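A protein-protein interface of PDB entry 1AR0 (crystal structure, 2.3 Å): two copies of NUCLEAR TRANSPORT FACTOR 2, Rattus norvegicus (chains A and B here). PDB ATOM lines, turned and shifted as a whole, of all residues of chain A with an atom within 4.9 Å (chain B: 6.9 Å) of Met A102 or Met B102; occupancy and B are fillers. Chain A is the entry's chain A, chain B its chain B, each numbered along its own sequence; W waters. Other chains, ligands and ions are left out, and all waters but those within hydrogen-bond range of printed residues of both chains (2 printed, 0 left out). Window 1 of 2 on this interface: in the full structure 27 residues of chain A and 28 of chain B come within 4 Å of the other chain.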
ATOM      1  N   ILE A  82       9.668 -16.242   4.685  1.00  0.00           N
ATOM      2  CA  ILE A  82       9.745 -17.275   5.716  1.00  0.00           C
ATOM      3  C   ILE A  82       8.731 -16.985   6.803  1.00  0.00           C
ATOM      4  O   ILE A  82       8.628 -15.867   7.295  1.00  0.00           O
ATOM      5  CB  ILE A  82      11.176 -17.465   6.206  1.00  0.00           C
ATOM      6  CG1 ILE A  82      11.305 -18.792   6.957  1.00  0.00           C
ATOM      7  CG2 ILE A  82      11.699 -16.330   7.038  1.00  0.00           C
ATOM      8  CD1 ILE A  82      12.732 -19.207   7.237  1.00  0.00           C
ATOM      9  N   SER A  83       7.907 -17.971   7.128  1.00  0.00           N
ATOM     10  CA  SER A  83       6.864 -17.860   8.122  1.00  0.00           C
ATOM     11  C   SER A  83       7.001 -18.887   9.262  1.00  0.00           C
ATOM     12  O   SER A  83       7.410 -20.012   9.021  1.00  0.00           O
ATOM     13  CB  SER A  83       5.477 -18.087   7.518  1.00  0.00           C
ATOM     14  OG  SER A  83       5.278 -17.226   6.415  1.00  0.00           O
ATOM     15  N   MET A  84       6.619 -18.476  10.468  1.00  0.00           N
ATOM     16  CA  MET A  84       6.579 -19.313  11.652  1.00  0.00           C
ATOM     17  C   MET A  84       5.210 -19.182  12.319  1.00  0.00           C
ATOM     18  O   MET A  84       4.723 -18.106  12.609  1.00  0.00           O
ATOM     19  CB  MET A  84       7.635 -19.023  12.709  1.00  0.00           C
ATOM     20  CG  MET A  84       7.618 -20.048  13.848  1.00  0.00           C
ATOM     21  SD  MET A  84       9.023 -19.966  14.961  1.00  0.00           S
ATOM     22  CE  MET A  84       8.502 -18.661  16.054  1.00  0.00           C
ATOM     23  N   HIS A 100       3.897 -26.434  16.243  1.00  0.00           N
ATOM     24  CA  HIS A 100       4.628 -25.336  15.631  1.00  0.00           C
ATOM     25  C   HIS A 100       4.880 -25.767  14.170  1.00  0.00           C
ATOM     26  O   HIS A 100       4.990 -26.962  13.932  1.00  0.00           O
ATOM     27  CB  HIS A 100       5.853 -24.872  16.313  1.00  0.00           C
ATOM     28  CG  HIS A 100       7.113 -25.619  16.292  1.00  0.00           C
ATOM     29  ND1 HIS A 100       8.209 -25.156  16.950  1.00  0.00           N
ATOM     30  CD2 HIS A 100       7.578 -26.756  15.762  1.00  0.00           C
ATOM     31  CE1 HIS A 100       9.239 -25.933  16.878  1.00  0.00           C
ATOM     32  NE2 HIS A 100       8.877 -26.933  16.116  1.00  0.00           N
ATOM     33  N   GLN A 101       4.839 -24.809  13.267  1.00  0.00           N
ATOM     34  CA  GLN A 101       5.044 -25.060  11.851  1.00  0.00           C
ATOM     35  C   GLN A 101       5.801 -23.900  11.207  1.00  0.00           C
ATOM     36  O   GLN A 101       5.696 -22.722  11.536  1.00  0.00           O
ATOM     37  CB  GLN A 101       3.731 -25.335  11.166  1.00  0.00           C
ATOM     38  CG  GLN A 101       3.856 -25.809   9.713  1.00  0.00           C
ATOM     39  CD  GLN A 101       2.693 -26.661   9.313  1.00  0.00           C
ATOM     40  OE1 GLN A 101       1.613 -26.504   9.872  1.00  0.00           O
ATOM     41  NE2 GLN A 101       2.871 -27.541   8.340  1.00  0.00           N
ATOM     42  N   MET A 102       6.638 -24.234  10.249  1.00  0.00           N
ATOM     43  CA  MET A 102       7.425 -23.235   9.522  1.00  0.00           C
ATOM     44  C   MET A 102       7.205 -23.471   8.055  1.00  0.00           C
ATOM     45  O   MET A 102       7.117 -24.604   7.581  1.00  0.00           O
ATOM     46  CB  MET A 102       8.866 -23.381   9.933  1.00  0.00           C
ATOM     47  CG  MET A 102       9.960 -22.808   9.116  1.00  0.00           C
ATOM     48  SD  MET A 102      10.328 -23.623   7.527  1.00  0.00           S
ATOM     49  CE  MET A 102      11.158 -22.245   6.819  1.00  0.00           C
ATOM     50  N   PHE A 103       7.113 -22.404   7.257  1.00  0.00           N
ATOM     51  CA  PHE A 103       6.966 -22.465   5.806  1.00  0.00           C
ATOM     52  C   PHE A 103       7.933 -21.502   5.132  1.00  0.00           C
ATOM     53  O   PHE A 103       8.230 -20.417   5.633  1.00  0.00           O
ATOM     54  CB  PHE A 103       5.615 -22.097   5.241  1.00  0.00           C
ATOM     55  CG  PHE A 103       4.427 -22.844   5.758  1.00  0.00           C
ATOM     56  CD1 PHE A 103       4.064 -24.071   5.274  1.00  0.00           C
ATOM     57  CD2 PHE A 103       3.763 -22.311   6.849  1.00  0.00           C
ATOM     58  CE1 PHE A 103       2.964 -24.715   5.807  1.00  0.00           C
ATOM     59  CE2 PHE A 103       2.659 -22.955   7.377  1.00  0.00           C
ATOM     60  CZ  PHE A 103       2.266 -24.161   6.857  1.00  0.00           C
ATOM     61  N   LEU A 104       8.614 -21.975   4.091  1.00  0.00           N
ATOM     62  CA  LEU A 104       9.526 -21.125   3.314  1.00  0.00           C
ATOM     63  C   LEU A 104       8.904 -21.012   1.920  1.00  0.00           C
ATOM     64  O   LEU A 104       8.721 -22.047   1.290  1.00  0.00           O
ATOM     65  CB  LEU A 104      10.952 -21.627   3.209  1.00  0.00           C
ATOM     66  CG  LEU A 104      11.888 -20.739   2.365  1.00  0.00           C
ATOM     67  CD1 LEU A 104      12.254 -19.457   3.115  1.00  0.00           C
ATOM     68  CD2 LEU A 104      13.183 -21.426   1.979  1.00  0.00           C
ATOM     69  N   ASN A 116       9.775 -25.445   1.504  1.00  0.00           N
ATOM     70  CA  ASN A 116      10.203 -26.100   2.740  1.00  0.00           C
ATOM     71  C   ASN A 116       9.121 -25.948   3.804  1.00  0.00           C
ATOM     72  O   ASN A 116       8.597 -24.853   3.998  1.00  0.00           O
ATOM     73  CB  ASN A 116      11.487 -25.555   3.293  1.00  0.00           C
ATOM     74  CG  ASN A 116      12.784 -25.817   2.574  1.00  0.00           C
ATOM     75  OD1 ASN A 116      13.517 -26.769   2.791  1.00  0.00           O
ATOM     76  ND2 ASN A 116      12.990 -24.917   1.616  1.00  0.00           N
ATOM     77  N   ASP A 117       8.714 -27.040   4.390  1.00  0.00           N
ATOM     78  CA  ASP A 117       7.660 -27.179   5.374  1.00  0.00           C
ATOM     79  C   ASP A 117       8.086 -28.099   6.515  1.00  0.00           C
ATOM     80  O   ASP A 117       8.504 -29.247   6.303  1.00  0.00           O
ATOM     81  CB  ASP A 117       6.444 -27.760   4.694  1.00  0.00           C
ATOM     82  CG  ASP A 117       5.210 -27.855   5.543  1.00  0.00           C
ATOM     83  OD1 ASP A 117       5.166 -27.584   6.758  1.00  0.00           O
ATOM     84  OD2 ASP A 117       4.180 -28.224   4.952  1.00  0.00           O
ATOM     85  N   MET A 118       8.045 -27.594   7.734  1.00  0.00           N
ATOM     86  CA  MET A 118       8.418 -28.341   8.926  1.00  0.00           C
ATOM     87  C   MET A 118       7.317 -28.245  10.004  1.00  0.00           C
ATOM     88  O   MET A 118       6.920 -27.150  10.383  1.00  0.00           O
ATOM     89  CB  MET A 118       9.697 -27.879   9.594  1.00  0.00           C
ATOM     90  CG  MET A 118      11.015 -28.109   8.894  1.00  0.00           C
ATOM     91  SD  MET A 118      12.346 -27.432   9.877  1.00  0.00           S
ATOM     92  CE  MET A 118      13.522 -26.973   8.660  1.00  0.00           C
ATOM     93  N   TYR B  19      22.989 -21.061  21.439  1.00  0.00           N
ATOM     94  CA  TYR B  19      22.589 -21.207  22.840  1.00  0.00           C
ATOM     95  C   TYR B  19      23.713 -21.158  23.847  1.00  0.00           C
ATOM     96  O   TYR B  19      23.525 -20.579  24.913  1.00  0.00           O
ATOM     97  CB  TYR B  19      21.703 -22.440  23.064  1.00  0.00           C
ATOM     98  CG  TYR B  19      20.395 -22.239  22.316  1.00  0.00           C
ATOM     99  CD1 TYR B  19      19.493 -21.260  22.718  1.00  0.00           C
ATOM    100  CD2 TYR B  19      20.103 -23.010  21.210  1.00  0.00           C
ATOM    101  CE1 TYR B  19      18.331 -21.081  22.015  1.00  0.00           C
ATOM    102  CE2 TYR B  19      18.940 -22.826  20.503  1.00  0.00           C
ATOM    103  CZ  TYR B  19      18.060 -21.855  20.914  1.00  0.00           C
ATOM    104  OH  TYR B  19      16.892 -21.661  20.232  1.00  0.00           O
ATOM    105  N   GLN B  74      16.595 -28.495   7.831  1.00  0.00           N
ATOM    106  CA  GLN B  74      16.407 -28.770   6.431  1.00  0.00           C
ATOM    107  C   GLN B  74      17.249 -27.872   5.528  1.00  0.00           C
ATOM    108  O   GLN B  74      17.435 -26.696   5.784  1.00  0.00           O
ATOM    109  CB  GLN B  74      14.989 -28.567   5.935  1.00  0.00           C
ATOM    110  CG  GLN B  74      13.868 -29.530   6.232  1.00  0.00           C
ATOM    111  CD  GLN B  74      12.538 -29.085   5.727  1.00  0.00           C
ATOM    112  OE1 GLN B  74      12.401 -27.951   5.254  1.00  0.00           O
ATOM    113  NE2 GLN B  74      11.530 -29.913   5.819  1.00  0.00           N
ATOM    114  N   THR B  76      17.533 -25.808   1.906  1.00  0.00           N
ATOM    115  CA  THR B  76      16.584 -25.177   0.977  1.00  0.00           C
ATOM    116  C   THR B  76      17.201 -25.332  -0.403  1.00  0.00           C
ATOM    117  O   THR B  76      18.410 -25.485  -0.590  1.00  0.00           O
ATOM    118  CB  THR B  76      16.402 -23.677   1.241  1.00  0.00           C
ATOM    119  OG1 THR B  76      17.626 -23.006   0.839  1.00  0.00           O
ATOM    120  CG2 THR B  76      16.161 -23.386   2.720  1.00  0.00           C
ATOM    121  N   ILE B  82      17.458 -24.233   7.205  1.00  0.00           N
ATOM    122  CA  ILE B  82      16.422 -23.853   8.132  1.00  0.00           C
ATOM    123  C   ILE B  82      16.539 -24.777   9.360  1.00  0.00           C
ATOM    124  O   ILE B  82      16.558 -26.006   9.212  1.00  0.00           O
ATOM    125  CB  ILE B  82      15.009 -23.952   7.598  1.00  0.00           C
ATOM    126  CG1 ILE B  82      14.804 -23.180   6.298  1.00  0.00           C
ATOM    127  CG2 ILE B  82      13.996 -23.388   8.600  1.00  0.00           C
ATOM    128  CD1 ILE B  82      13.820 -23.878   5.410  1.00  0.00           C
ATOM    129  N   SER B  83      16.653 -24.214  10.536  1.00  0.00           N
ATOM    130  CA  SER B  83      16.726 -24.918  11.798  1.00  0.00           C
ATOM    131  C   SER B  83      15.534 -24.515  12.661  1.00  0.00           C
ATOM    132  O   SER B  83      15.322 -23.344  12.896  1.00  0.00           O
ATOM    133  CB  SER B  83      17.959 -24.539  12.587  1.00  0.00           C
ATOM    134  OG  SER B  83      19.146 -24.843  11.883  1.00  0.00           O
ATOM    135  N   MET B  84      14.784 -25.472  13.144  1.00  0.00           N
ATOM    136  CA  MET B  84      13.642 -25.226  13.998  1.00  0.00           C
ATOM    137  C   MET B  84      13.773 -25.970  15.328  1.00  0.00           C
ATOM    138  O   MET B  84      14.104 -27.141  15.423  1.00  0.00           O
ATOM    139  CB  MET B  84      12.380 -25.610  13.257  1.00  0.00           C
ATOM    140  CG  MET B  84      11.202 -25.128  14.078  1.00  0.00           C
ATOM    141  SD  MET B  84       9.861 -24.573  13.056  1.00  0.00           S
ATOM    142  CE  MET B  84       9.067 -26.082  12.634  1.00  0.00           C
ATOM    143  N   VAL B  85      13.646 -25.275  16.443  1.00  0.00           N
ATOM    144  CA  VAL B  85      13.873 -25.754  17.793  1.00  0.00           C
ATOM    145  C   VAL B  85      12.643 -25.561  18.675  1.00  0.00           C
ATOM    146  O   VAL B  85      12.012 -24.505  18.673  1.00  0.00           O
ATOM    147  CB  VAL B  85      15.045 -25.003  18.459  1.00  0.00           C
ATOM    148  CG1 VAL B  85      15.219 -25.151  19.964  1.00  0.00           C
ATOM    149  CG2 VAL B  85      16.415 -25.411  17.907  1.00  0.00           C
ATOM    150  N   HIS B 100       9.735 -21.610  21.316  1.00  0.00           N
ATOM    151  CA  HIS B 100       9.846 -22.021  19.930  1.00  0.00           C
ATOM    152  C   HIS B 100      10.815 -21.046  19.233  1.00  0.00           C
ATOM    153  O   HIS B 100      10.679 -19.828  19.386  1.00  0.00           O
ATOM    154  CB  HIS B 100       8.578 -22.006  19.072  1.00  0.00           C
ATOM    155  CG  HIS B 100       7.470 -22.807  19.650  1.00  0.00           C
ATOM    156  ND1 HIS B 100       6.585 -22.273  20.571  1.00  0.00           N
ATOM    157  CD2 HIS B 100       7.166 -24.101  19.638  1.00  0.00           C
ATOM    158  CE1 HIS B 100       5.748 -23.193  20.977  1.00  0.00           C
ATOM    159  NE2 HIS B 100       6.087 -24.331  20.405  1.00  0.00           N
ATOM    160  N   GLN B 101      11.776 -21.586  18.512  1.00  0.00           N
ATOM    161  CA  GLN B 101      12.689 -20.708  17.796  1.00  0.00           C
ATOM    162  C   GLN B 101      13.026 -21.334  16.432  1.00  0.00           C
ATOM    163  O   GLN B 101      13.126 -22.542  16.252  1.00  0.00           O
ATOM    164  CB  GLN B 101      13.921 -20.319  18.561  1.00  0.00           C
ATOM    165  CG  GLN B 101      14.677 -19.103  18.083  1.00  0.00           C
ATOM    166  CD  GLN B 101      15.624 -18.516  19.099  1.00  0.00           C
ATOM    167  OE1 GLN B 101      15.908 -19.170  20.116  1.00  0.00           O
ATOM    168  NE2 GLN B 101      16.132 -17.292  18.912  1.00  0.00           N
ATOM    169  N   MET B 102      13.193 -20.426  15.473  1.00  0.00           N
ATOM    170  CA  MET B 102      13.504 -20.743  14.086  1.00  0.00           C
ATOM    171  C   MET B 102      14.561 -19.806  13.535  1.00  0.00           C
ATOM    172  O   MET B 102      14.684 -18.622  13.838  1.00  0.00           O
ATOM    173  CB  MET B 102      12.279 -20.693  13.203  1.00  0.00           C
ATOM    174  CG  MET B 102      12.555 -21.134  11.764  1.00  0.00           C
ATOM    175  SD  MET B 102      12.554 -19.660  10.677  1.00  0.00           S
ATOM    176  CE  MET B 102      10.793 -19.641  10.439  1.00  0.00           C
ATOM    177  N   PHE B 103      15.527 -20.428  12.841  1.00  0.00           N
ATOM    178  CA  PHE B 103      16.686 -19.810  12.264  1.00  0.00           C
ATOM    179  C   PHE B 103      16.857 -20.096  10.775  1.00  0.00           C
ATOM    180  O   PHE B 103      16.706 -21.236  10.333  1.00  0.00           O
ATOM    181  CB  PHE B 103      17.990 -20.265  12.928  1.00  0.00           C
ATOM    182  CG  PHE B 103      18.090 -20.196  14.426  1.00  0.00           C
ATOM    183  CD1 PHE B 103      18.398 -19.020  15.064  1.00  0.00           C
ATOM    184  CD2 PHE B 103      17.753 -21.311  15.193  1.00  0.00           C
ATOM    185  CE1 PHE B 103      18.448 -18.984  16.450  1.00  0.00           C
ATOM    186  CE2 PHE B 103      17.801 -21.258  16.577  1.00  0.00           C
ATOM    187  CZ  PHE B 103      18.164 -20.092  17.198  1.00  0.00           C
ATOM    188  N   LEU B 104      17.155 -19.052   9.989  1.00  0.00           N
ATOM    189  CA  LEU B 104      17.454 -19.264   8.566  1.00  0.00           C
ATOM    190  C   LEU B 104      18.941 -18.976   8.427  1.00  0.00           C
ATOM    191  O   LEU B 104      19.354 -17.908   8.850  1.00  0.00           O
ATOM    192  CB  LEU B 104      16.663 -18.440   7.578  1.00  0.00           C
ATOM    193  CG  LEU B 104      16.956 -18.727   6.091  1.00  0.00           C
ATOM    194  CD1 LEU B 104      16.574 -20.126   5.682  1.00  0.00           C
ATOM    195  CD2 LEU B 104      16.170 -17.766   5.199  1.00  0.00           C
ATOM    196  N   CYS B 114      23.370 -16.391  10.603  1.00  0.00           N
ATOM    197  CA  CYS B 114      21.929 -16.393  10.705  1.00  0.00           C
ATOM    198  C   CYS B 114      21.338 -15.165  10.037  1.00  0.00           C
ATOM    199  O   CYS B 114      21.687 -14.053  10.442  1.00  0.00           O
ATOM    200  CB  CYS B 114      21.517 -16.368  12.200  1.00  0.00           C
ATOM    201  SG  CYS B 114      19.705 -16.380  12.305  1.00  0.00           S
ATOM    202  N   ASN B 116      17.831 -14.708   9.465  1.00  0.00           N
ATOM    203  CA  ASN B 116      16.455 -14.580   9.926  1.00  0.00           C
ATOM    204  C   ASN B 116      16.262 -15.387  11.217  1.00  0.00           C
ATOM    205  O   ASN B 116      16.691 -16.544  11.335  1.00  0.00           O
ATOM    206  CB  ASN B 116      15.459 -15.046   8.873  1.00  0.00           C
ATOM    207  CG  ASN B 116      15.337 -14.180   7.616  1.00  0.00           C
ATOM    208  OD1 ASN B 116      14.536 -13.291   7.421  1.00  0.00           O
ATOM    209  ND2 ASN B 116      16.306 -14.435   6.715  1.00  0.00           N
ATOM    210  N   ASP B 117      15.684 -14.764  12.234  1.00  0.00           N
ATOM    211  CA  ASP B 117      15.517 -15.360  13.560  1.00  0.00           C
ATOM    212  C   ASP B 117      14.166 -15.017  14.138  1.00  0.00           C
ATOM    213  O   ASP B 117      13.759 -13.858  14.205  1.00  0.00           O
ATOM    214  CB  ASP B 117      16.645 -14.918  14.462  1.00  0.00           C
ATOM    215  CG  ASP B 117      16.685 -15.450  15.883  1.00  0.00           C
ATOM    216  OD1 ASP B 117      15.798 -16.167  16.362  1.00  0.00           O
ATOM    217  OD2 ASP B 117      17.642 -15.135  16.616  1.00  0.00           O
ATOM    218  N   MET B 118      13.373 -16.025  14.474  1.00  0.00           N
ATOM    219  CA  MET B 118      12.052 -15.836  15.045  1.00  0.00           C
ATOM    220  C   MET B 118      11.960 -16.601  16.382  1.00  0.00           C
ATOM    221  O   MET B 118      12.269 -17.795  16.453  1.00  0.00           O
ATOM    222  CB  MET B 118      10.936 -16.250  14.093  1.00  0.00           C
ATOM    223  CG  MET B 118      10.674 -15.314  12.920  1.00  0.00           C
ATOM    224  SD  MET B 118       9.471 -15.886  11.761  1.00  0.00           S
ATOM    225  CE  MET B 118      10.196 -15.657  10.166  1.00  0.00           C
ATOM    226  N   PHE B 119      11.483 -15.939  17.419  1.00  0.00           N
ATOM    227  CA  PHE B 119      11.357 -16.492  18.757  1.00  0.00           C
ATOM    228  C   PHE B 119       9.971 -16.254  19.333  1.00  0.00           C
ATOM    229  O   PHE B 119       9.497 -15.113  19.358  1.00  0.00           O
ATOM    230  CB  PHE B 119      12.409 -15.910  19.703  1.00  0.00           C
ATOM    231  CG  PHE B 119      12.286 -16.288  21.162  1.00  0.00           C
ATOM    232  CD1 PHE B 119      12.851 -17.456  21.633  1.00  0.00           C
ATOM    233  CD2 PHE B 119      11.619 -15.471  22.077  1.00  0.00           C
ATOM    234  CE1 PHE B 119      12.736 -17.828  22.968  1.00  0.00           C
ATOM    235  CE2 PHE B 119      11.502 -15.845  23.410  1.00  0.00           C
ATOM    236  CZ  PHE B 119      12.064 -17.021  23.866  1.00  0.00           C
ATOM    237  N   ARG B 120       9.410 -17.280  19.946  1.00  0.00           N
ATOM    238  CA  ARG B 120       8.117 -17.165  20.609  1.00  0.00           C
ATOM    239  C   ARG B 120       8.131 -18.006  21.895  1.00  0.00           C
ATOM    240  O   ARG B 120       8.603 -19.134  21.847  1.00  0.00           O
ATOM    241  CB  ARG B 120       6.946 -17.744  19.844  1.00  0.00           C
ATOM    242  CG  ARG B 120       6.313 -17.019  18.693  1.00  0.00           C
ATOM    243  CD  ARG B 120       5.212 -16.084  19.092  1.00  0.00           C
ATOM    244  NE  ARG B 120       4.945 -15.073  18.070  1.00  0.00           N
ATOM    245  CZ  ARG B 120       4.203 -13.998  18.323  1.00  0.00           C
ATOM    246  NH1 ARG B 120       3.669 -13.810  19.536  1.00  0.00           N
ATOM    247  NH2 ARG B 120       3.972 -13.117  17.369  1.00  0.00           N
HETATM  248  O   HOH W   1       8.808 -22.900  15.843  1.00  0.00           O
HETATM  249  O   HOH W   2      11.661 -28.711  16.093  1.00  0.00           O
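Of the printed residues of chain B, Met A102 touches Ile B82, Met B84 and Met B102. Of the printed residues of chain A, Thr B76 touches Leu A104 (3.6 Å) and Asn A116 (3.6 Å). Printed residues of chain A within 4 Å of Gln B74: Asn A116 (3.0 Å), Asp A117 (3.1 Å) and Met A118 (3.5 Å). Leu B104 touches none of the printed residues of chain A.
Of the 11 printed residues of chain A, 9 touch a printed residue of chain B. Hydrophobic or aromatic side chains of chain A within 4 Å of the printed part of chain B: Ile A82, Met A84, His A100, Met A102, Leu A104 and Met A118. Among the printed residues, no Asp or Glu carboxylate lies within 4 Å of a Lys or Arg side-chain nitrogen of the other chain.
The side-chain carboxylate (OD1) of Asp A117 lies within hydrogen-bond range of the side-chain amide nitrogen (NE2) of Gln A101 (2.8 Å). The backbone NH (N) of Leu A104 sits at hydrogen-bond distance from the backbone carbonyl oxygen (O) of Asn A116 (2.9 Å). The backbone NH of His B100 sits at hydrogen-bond distance from the backbone carbonyl oxygen of Arg B120, 2.8 Å away. N of Met B102 sits at hydrogen-bond distance from O of Met B118 (3.0 Å). The backbone carbonyl oxygen of Phe A103 sits at hydrogen-bond distance from the backbone NH of Ser A83 (2.9 Å). N of Ile B82 sits at hydrogen-bond distance from O of Gln B74 (2.8 Å).
Met A84 touches Met B102, and with the chains exchanged Met A102 touches Met B84. Met A84 touches Met B118, and with the chains exchanged Met A118 touches Met B84. His A100 touches Met B84, but with the chains exchanged Met A84 does not touch His B100 (4.1 Å). His B100 touches its own counterpart, His A100. Positions printed for both chains: 82, 83, 84, 100, 101, 102, 103, 104, 116, 117 and 118.
Water W1 lies within hydrogen-bond range of ND1 of His A100, SD of Met A84 and SD of Met B84. Water W2 bridges the backbone carbonyl oxygen of Met B84 (3.0 Å) and a ring nitrogen (NE2) of His A100 (3.3 Å).
Among the printed residues, merely in contact across the chains: Ile A82 with Met B102, Ile A82 with Met B118, Ser A83 with Met B102, Met A84 with Met B102, Met A84 with Met B118, Met A84 with Arg B120, His A100 with Met B84, His A100 with Val B85, His A100 with His B100, Met A102 with Ile B82, Met A102 with Met B84, Met A102 with Met B102, Leu A104 with Thr B76, Asn A116 with Thr B76, Asn A116 with Ile B82, Met A118 with Gln B74, Met A118 with Ile B82 and Met A118 with Met B84.
O of Asp A117 sits at hydrogen-bond distance from NE2 of Gln B74. OE1 of Gln B74 lies close to OD1 of Asn A116 (3.0 Å).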
